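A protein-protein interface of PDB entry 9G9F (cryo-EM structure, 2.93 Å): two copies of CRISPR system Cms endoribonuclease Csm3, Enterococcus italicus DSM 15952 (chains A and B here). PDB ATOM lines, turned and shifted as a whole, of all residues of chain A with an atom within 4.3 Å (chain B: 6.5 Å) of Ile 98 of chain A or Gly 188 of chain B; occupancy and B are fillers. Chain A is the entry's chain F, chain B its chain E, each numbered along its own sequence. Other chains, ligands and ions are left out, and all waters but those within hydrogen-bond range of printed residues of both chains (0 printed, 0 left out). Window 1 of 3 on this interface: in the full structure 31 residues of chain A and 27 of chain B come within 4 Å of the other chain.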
ATOM      1  N   GLY A  48     -12.060 -12.556  25.337  1.00  0.00           N
ATOM      2  CA  GLY A  48     -13.243 -13.280  24.911  1.00  0.00           C
ATOM      3  C   GLY A  48     -14.292 -12.366  24.316  1.00  0.00           C
ATOM      4  O   GLY A  48     -15.007 -12.746  23.387  1.00  0.00           O
ATOM      5  N   ILE A  51     -13.446 -11.741  20.625  1.00  0.00           N
ATOM      6  CA  ILE A  51     -13.755 -12.896  19.784  1.00  0.00           C
ATOM      7  C   ILE A  51     -15.260 -13.031  19.597  1.00  0.00           C
ATOM      8  O   ILE A  51     -15.747 -13.259  18.486  1.00  0.00           O
ATOM      9  CB  ILE A  51     -13.146 -14.174  20.386  1.00  0.00           C
ATOM     10  CG1 ILE A  51     -11.628 -14.051  20.470  1.00  0.00           C
ATOM     11  CG2 ILE A  51     -13.526 -15.380  19.557  1.00  0.00           C
ATOM     12  CD1 ILE A  51     -10.949 -15.290  20.984  1.00  0.00           C
ATOM     13  N   LYS A  52     -16.020 -12.887  20.686  1.00  0.00           N
ATOM     14  CA  LYS A  52     -17.468 -13.032  20.598  1.00  0.00           C
ATOM     15  C   LYS A  52     -18.083 -11.942  19.733  1.00  0.00           C
ATOM     16  O   LYS A  52     -18.940 -12.225  18.889  1.00  0.00           O
ATOM     17  CB  LYS A  52     -18.089 -13.015  21.992  1.00  0.00           C
ATOM     18  CG  LYS A  52     -19.515 -13.533  22.009  1.00  0.00           C
ATOM     19  CD  LYS A  52     -20.351 -12.916  23.102  1.00  0.00           C
ATOM     20  CE  LYS A  52     -21.764 -13.455  23.031  1.00  0.00           C
ATOM     21  NZ  LYS A  52     -22.686 -12.748  23.945  1.00  0.00           N
ATOM     22  N   MET A  55     -17.153 -12.604  16.040  1.00  0.00           N
ATOM     23  CA  MET A  55     -17.883 -13.740  15.490  1.00  0.00           C
ATOM     24  C   MET A  55     -19.349 -13.398  15.261  1.00  0.00           C
ATOM     25  O   MET A  55     -19.912 -13.735  14.213  1.00  0.00           O
ATOM     26  CB  MET A  55     -17.749 -14.946  16.418  1.00  0.00           C
ATOM     27  CG  MET A  55     -16.688 -15.941  15.988  1.00  0.00           C
ATOM     28  SD  MET A  55     -16.469 -17.273  17.178  1.00  0.00           S
ATOM     29  CE  MET A  55     -18.170 -17.740  17.470  1.00  0.00           C
ATOM     30  N   PHE A  83     -25.782 -16.424  20.830  1.00  0.00           N
ATOM     31  CA  PHE A  83     -25.001 -15.458  21.585  1.00  0.00           C
ATOM     32  C   PHE A  83     -25.801 -14.677  22.614  1.00  0.00           C
ATOM     33  O   PHE A  83     -25.209 -14.172  23.571  1.00  0.00           O
ATOM     34  CB  PHE A  83     -24.321 -14.464  20.633  1.00  0.00           C
ATOM     35  CG  PHE A  83     -23.320 -15.096  19.711  1.00  0.00           C
ATOM     36  CD1 PHE A  83     -22.074 -15.475  20.176  1.00  0.00           C
ATOM     37  CD2 PHE A  83     -23.623 -15.311  18.379  1.00  0.00           C
ATOM     38  CE1 PHE A  83     -21.153 -16.055  19.330  1.00  0.00           C
ATOM     39  CE2 PHE A  83     -22.704 -15.892  17.530  1.00  0.00           C
ATOM     40  CZ  PHE A  83     -21.470 -16.264  18.006  1.00  0.00           C
ATOM     41  N   LEU A  96     -23.522 -19.453  24.122  1.00  0.00           N
ATOM     42  CA  LEU A  96     -22.099 -19.501  23.821  1.00  0.00           C
ATOM     43  C   LEU A  96     -21.363 -18.500  24.695  1.00  0.00           C
ATOM     44  O   LEU A  96     -21.660 -17.303  24.658  1.00  0.00           O
ATOM     45  CB  LEU A  96     -21.840 -19.213  22.345  1.00  0.00           C
ATOM     46  CG  LEU A  96     -20.633 -19.960  21.787  1.00  0.00           C
ATOM     47  CD1 LEU A  96     -20.783 -21.439  22.086  1.00  0.00           C
ATOM     48  CD2 LEU A  96     -20.479 -19.725  20.298  1.00  0.00           C
ATOM     49  N   GLN A  97     -20.399 -18.988  25.470  1.00  0.00           N
ATOM     50  CA  GLN A  97     -19.639 -18.175  26.417  1.00  0.00           C
ATOM     51  C   GLN A  97     -18.160 -18.277  26.059  1.00  0.00           C
ATOM     52  O   GLN A  97     -17.428 -19.094  26.618  1.00  0.00           O
ATOM     53  CB  GLN A  97     -19.906 -18.641  27.836  1.00  0.00           C
ATOM     54  CG  GLN A  97     -21.370 -18.889  28.133  1.00  0.00           C
ATOM     55  CD  GLN A  97     -21.594 -19.435  29.523  1.00  0.00           C
ATOM     56  OE1 GLN A  97     -20.654 -19.588  30.298  1.00  0.00           O
ATOM     57  NE2 GLN A  97     -22.845 -19.733  29.848  1.00  0.00           N
ATOM     58  N   ILE A  98     -17.718 -17.429  25.133  1.00  0.00           N
ATOM     59  CA  ILE A  98     -16.329 -17.437  24.688  1.00  0.00           C
ATOM     60  C   ILE A  98     -15.477 -16.636  25.658  1.00  0.00           C
ATOM     61  O   ILE A  98     -15.810 -15.498  25.999  1.00  0.00           O
ATOM     62  CB  ILE A  98     -16.212 -16.899  23.255  1.00  0.00           C
ATOM     63  CG1 ILE A  98     -17.337 -17.471  22.392  1.00  0.00           C
ATOM     64  CG2 ILE A  98     -14.848 -17.209  22.674  1.00  0.00           C
ATOM     65  CD1 ILE A  98     -17.886 -16.529  21.380  1.00  0.00           C
ATOM     66  N   SER A  99     -14.377 -17.230  26.104  1.00  0.00           N
ATOM     67  CA  SER A  99     -13.529 -16.659  27.139  1.00  0.00           C
ATOM     68  C   SER A  99     -12.214 -16.166  26.553  1.00  0.00           C
ATOM     69  O   SER A  99     -11.950 -16.280  25.354  1.00  0.00           O
ATOM     70  CB  SER A  99     -13.262 -17.681  28.248  1.00  0.00           C
ATOM     71  OG  SER A  99     -12.297 -18.633  27.842  1.00  0.00           O
ATOM     72  N   ASP A 100     -11.383 -15.617  27.436  1.00  0.00           N
ATOM     73  CA  ASP A 100     -10.121 -15.015  27.032  1.00  0.00           C
ATOM     74  C   ASP A 100      -9.156 -16.071  26.513  1.00  0.00           C
ATOM     75  O   ASP A 100      -9.114 -17.199  27.010  1.00  0.00           O
ATOM     76  CB  ASP A 100      -9.493 -14.265  28.207  1.00  0.00           C
ATOM     77  CG  ASP A 100     -10.382 -13.151  28.742  1.00  0.00           C
ATOM     78  OD1 ASP A 100     -11.561 -13.409  29.056  1.00  0.00           O
ATOM     79  OD2 ASP A 100      -9.897 -12.010  28.863  1.00  0.00           O
ATOM     80  N   ILE A 152     -14.280 -22.185  24.795  1.00  0.00           N
ATOM     81  CA  ILE A 152     -15.690 -21.829  24.744  1.00  0.00           C
ATOM     82  C   ILE A 152     -16.488 -22.903  25.468  1.00  0.00           C
ATOM     83  O   ILE A 152     -16.063 -24.057  25.564  1.00  0.00           O
ATOM     84  CB  ILE A 152     -16.164 -21.675  23.286  1.00  0.00           C
ATOM     85  CG1 ILE A 152     -15.174 -20.840  22.482  1.00  0.00           C
ATOM     86  CG2 ILE A 152     -17.513 -21.025  23.232  1.00  0.00           C
ATOM     87  CD1 ILE A 152     -15.701 -20.451  21.120  1.00  0.00           C
ATOM     88  N   LEU B  14     -10.309 -17.484  36.570  1.00  0.00           N
ATOM     89  CA  LEU B  14      -9.519 -17.866  35.408  1.00  0.00           C
ATOM     90  C   LEU B  14      -9.564 -16.801  34.328  1.00  0.00           C
ATOM     91  O   LEU B  14      -8.791 -16.868  33.368  1.00  0.00           O
ATOM     92  CB  LEU B  14     -10.011 -19.196  34.844  1.00  0.00           C
ATOM     93  CG  LEU B  14      -9.987 -20.366  35.820  1.00  0.00           C
ATOM     94  CD1 LEU B  14     -10.263 -21.653  35.080  1.00  0.00           C
ATOM     95  CD2 LEU B  14      -8.656 -20.428  36.535  1.00  0.00           C
ATOM     96  N   THR B  15     -10.474 -15.841  34.451  1.00  0.00           N
ATOM     97  CA  THR B  15     -10.518 -14.687  33.567  1.00  0.00           C
ATOM     98  C   THR B  15     -10.922 -13.473  34.387  1.00  0.00           C
ATOM     99  O   THR B  15     -10.970 -13.541  35.619  1.00  0.00           O
ATOM    100  CB  THR B  15     -11.506 -14.897  32.424  1.00  0.00           C
ATOM    101  OG1 THR B  15     -12.636 -15.624  32.906  1.00  0.00           O
ATOM    102  CG2 THR B  15     -10.873 -15.686  31.307  1.00  0.00           C
ATOM    103  N   GLY B  16     -11.229 -12.367  33.721  1.00  0.00           N
ATOM    104  CA  GLY B  16     -11.748 -11.217  34.428  1.00  0.00           C
ATOM    105  C   GLY B  16     -13.085 -11.515  35.075  1.00  0.00           C
ATOM    106  O   GLY B  16     -13.841 -12.375  34.637  1.00  0.00           O
ATOM    107  N   ARG B 141     -12.908  -4.836  35.504  1.00  0.00           N
ATOM    108  CA  ARG B 141     -12.844  -6.266  35.754  1.00  0.00           C
ATOM    109  C   ARG B 141     -11.860  -6.555  36.881  1.00  0.00           C
ATOM    110  O   ARG B 141     -11.157  -5.671  37.364  1.00  0.00           O
ATOM    111  CB  ARG B 141     -12.433  -7.014  34.495  1.00  0.00           C
ATOM    112  CG  ARG B 141     -13.303  -6.752  33.300  1.00  0.00           C
ATOM    113  CD  ARG B 141     -13.042  -7.798  32.239  1.00  0.00           C
ATOM    114  NE  ARG B 141     -11.641  -8.200  32.214  1.00  0.00           N
ATOM    115  CZ  ARG B 141     -11.185  -9.291  31.615  1.00  0.00           C
ATOM    116  NH1 ARG B 141     -11.996 -10.123  30.985  1.00  0.00           N
ATOM    117  NH2 ARG B 141      -9.885  -9.557  31.657  1.00  0.00           N
ATOM    118  N   GLY B 184     -21.215  -9.986  32.407  1.00  0.00           N
ATOM    119  CA  GLY B 184     -20.317 -10.050  31.274  1.00  0.00           C
ATOM    120  C   GLY B 184     -19.701 -11.406  31.050  1.00  0.00           C
ATOM    121  O   GLY B 184     -18.760 -11.527  30.264  1.00  0.00           O
ATOM    122  N   GLY B 185     -20.212 -12.441  31.714  1.00  0.00           N
ATOM    123  CA  GLY B 185     -19.614 -13.755  31.588  1.00  0.00           C
ATOM    124  C   GLY B 185     -19.723 -14.322  30.191  1.00  0.00           C
ATOM    125  O   GLY B 185     -18.919 -15.165  29.794  1.00  0.00           O
ATOM    126  N   THR B 186     -20.713 -13.871  29.431  1.00  0.00           N
ATOM    127  CA  THR B 186     -20.857 -14.325  28.059  1.00  0.00           C
ATOM    128  C   THR B 186     -19.762 -13.785  27.150  1.00  0.00           C
ATOM    129  O   THR B 186     -19.591 -14.295  26.038  1.00  0.00           O
ATOM    130  CB  THR B 186     -22.226 -13.918  27.529  1.00  0.00           C
ATOM    131  OG1 THR B 186     -23.206 -14.139  28.549  1.00  0.00           O
ATOM    132  CG2 THR B 186     -22.582 -14.750  26.337  1.00  0.00           C
ATOM    133  N   ARG B 187     -19.023 -12.776  27.587  1.00  0.00           N
ATOM    134  CA  ARG B 187     -17.982 -12.156  26.783  1.00  0.00           C
ATOM    135  C   ARG B 187     -16.626 -12.282  27.464  1.00  0.00           C
ATOM    136  O   ARG B 187     -15.837 -11.339  27.507  1.00  0.00           O
ATOM    137  CB  ARG B 187     -18.322 -10.696  26.501  1.00  0.00           C
ATOM    138  CG  ARG B 187     -19.547 -10.517  25.620  1.00  0.00           C
ATOM    139  CD  ARG B 187     -19.997  -9.075  25.584  1.00  0.00           C
ATOM    140  NE  ARG B 187     -20.197  -8.535  26.923  1.00  0.00           N
ATOM    141  CZ  ARG B 187     -21.340  -8.587  27.590  1.00  0.00           C
ATOM    142  NH1 ARG B 187     -22.415  -9.155  27.076  1.00  0.00           N
ATOM    143  NH2 ARG B 187     -21.407  -8.055  28.805  1.00  0.00           N
ATOM    144  N   GLY B 188     -16.346 -13.460  28.012  1.00  0.00           N
ATOM    145  CA  GLY B 188     -15.046 -13.787  28.541  1.00  0.00           C
ATOM    146  C   GLY B 188     -14.922 -13.694  30.044  1.00  0.00           C
ATOM    147  O   GLY B 188     -14.002 -14.290  30.610  1.00  0.00           O
ATOM    148  N   ASN B 189     -15.822 -12.981  30.705  1.00  0.00           N
ATOM    149  CA  ASN B 189     -15.706 -12.794  32.138  1.00  0.00           C
ATOM    150  C   ASN B 189     -16.220 -14.019  32.886  1.00  0.00           C
ATOM    151  O   ASN B 189     -16.791 -14.946  32.311  1.00  0.00           O
ATOM    152  CB  ASN B 189     -16.479 -11.555  32.581  1.00  0.00           C
ATOM    153  CG  ASN B 189     -16.012 -10.299  31.887  1.00  0.00           C
ATOM    154  OD1 ASN B 189     -14.848 -10.182  31.522  1.00  0.00           O
ATOM    155  ND2 ASN B 189     -16.918  -9.350  31.705  1.00  0.00           N
ATOM    156  N   GLY B 190     -15.975 -14.025  34.191  1.00  0.00           N
ATOM    157  CA  GLY B 190     -16.671 -14.894  35.107  1.00  0.00           C
ATOM    158  C   GLY B 190     -16.077 -16.266  35.330  1.00  0.00           C
ATOM    159  O   GLY B 190     -16.445 -16.916  36.314  1.00  0.00           O
ATOM    160  N   ARG B 191     -15.180 -16.738  34.468  1.00  0.00           N
ATOM    161  CA  ARG B 191     -14.653 -18.087  34.635  1.00  0.00           C
ATOM    162  C   ARG B 191     -13.948 -18.216  35.975  1.00  0.00           C
ATOM    163  O   ARG B 191     -13.166 -17.345  36.362  1.00  0.00           O
ATOM    164  CB  ARG B 191     -13.694 -18.429  33.501  1.00  0.00           C
ATOM    165  CG  ARG B 191     -14.381 -18.833  32.216  1.00  0.00           C
ATOM    166  CD  ARG B 191     -13.406 -19.510  31.277  1.00  0.00           C
ATOM    167  NE  ARG B 191     -12.804 -20.693  31.877  1.00  0.00           N
ATOM    168  CZ  ARG B 191     -11.721 -21.295  31.409  1.00  0.00           C
ATOM    169  NH1 ARG B 191     -11.087 -20.840  30.341  1.00  0.00           N
ATOM    170  NH2 ARG B 191     -11.262 -22.377  32.028  1.00  0.00           N
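Along chain A the printed residues that touch a printed residue of chain B span positions 48 to 100. Printed residues of chain B that touch a printed residue of chain A: Thr 15, Arg 141, Thr 186, Arg 187, Gly 188 and Arg 191. Along chain B the printed residues that touch a printed residue of chain A span positions 15 to 191. Among the printed residues, Asp or Glu carboxylates within 4 Å of a Lys or Arg side-chain nitrogen of the other chain: Asp 100 of chain A with Arg 141 of chain B (3.5 Å).
No position is printed for both chains.
The side-chain carboxylate (OD1) of Asp 100 of chain A sits close to the backbone carbonyl oxygen (O) of Gly 188 of chain B (3.0 Å). O of Ile 98 of chain A sits at hydrogen-bond distance from N of Gly 188 of chain B (2.9 Å). OD2 of Asp 100 of chain A lies within salt-bridge range of NH1 of Arg 141 of chain B (3.5 Å).
Arg 187 of chain B touches Gly 48 of chain A (O to C, 3.7 Å). CG2 of Thr 186 of chain B touches NZ of Lys 52 of chain A, 3.1 Å away. Arg 187 of chain B touches Lys 52 of chain A. Leu 96 of chain A touches Thr 186 of chain B (O to CG2, 3.2 Å). Gln 97 of chain A touches Thr 186 of chain B. O of Thr 186 of chain B touches N of Ile 98 of chain A, 3.8 Å away. Arg 187 of chain B touches Ile 98 of chain A (C to O, 3.6 Å). Gly 188 of chain B touches Ser 99 of chain A. Arg 191 of chain B touches Ser 99 of chain A. OD1 of Asp 100 of chain A touches CG2 of Thr 15 of chain B (3.3 Å).
The side-chain amide oxygen (OD1) of Asn 189 of chain B is in hydrogen-bond range of the guanidinium group (NH1) of Arg 141 of chain B (2.9 Å). The side-chain hydroxyl (OG1) of Thr 15 of chain B lies within hydrogen-bond range of the backbone carbonyl oxygen (O) of Gly 188 of chain B (3.0 Å). OG1 of Thr 15 of chain B lies close to N of Arg 191 of chain B, at 3.2 Å. The backbone NH (N) of Leu 14 of chain B sits at hydrogen-bond distance from the backbone carbonyl oxygen (O) of Arg 191 of chain B (2.9 Å). NZ of Lys 52 of chain A is in hydrogen-bond range of O of Phe 83 of chain A, 2.9 Å away.
Ile 98 of chain A touches three residues of chain B. Of the printed residues of chain A, Gly 188 of chain B touches Ile 98 (2.9 Å), Ser 99 (3.5 Å) and Asp 100 (3.0 Å). Printed residues of chain A within 4 Å of Arg 191 of chain B: Ser 99. Printed residues of chain A within 4 Å of Arg 141 of chain B: Asp 100 (3.5 Å). Of the printed residues of chain B, Lys 52 of chain A touches Thr 186 and Arg 187. The nearest residue of chain A that does not touch Gly 188 of chain B is Gly 48 of chain A (4.1 Å). The nearest printed residue of chain B that does not touch Ser 99 of chain A is Thr 15 of chain B (4.4 Å).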
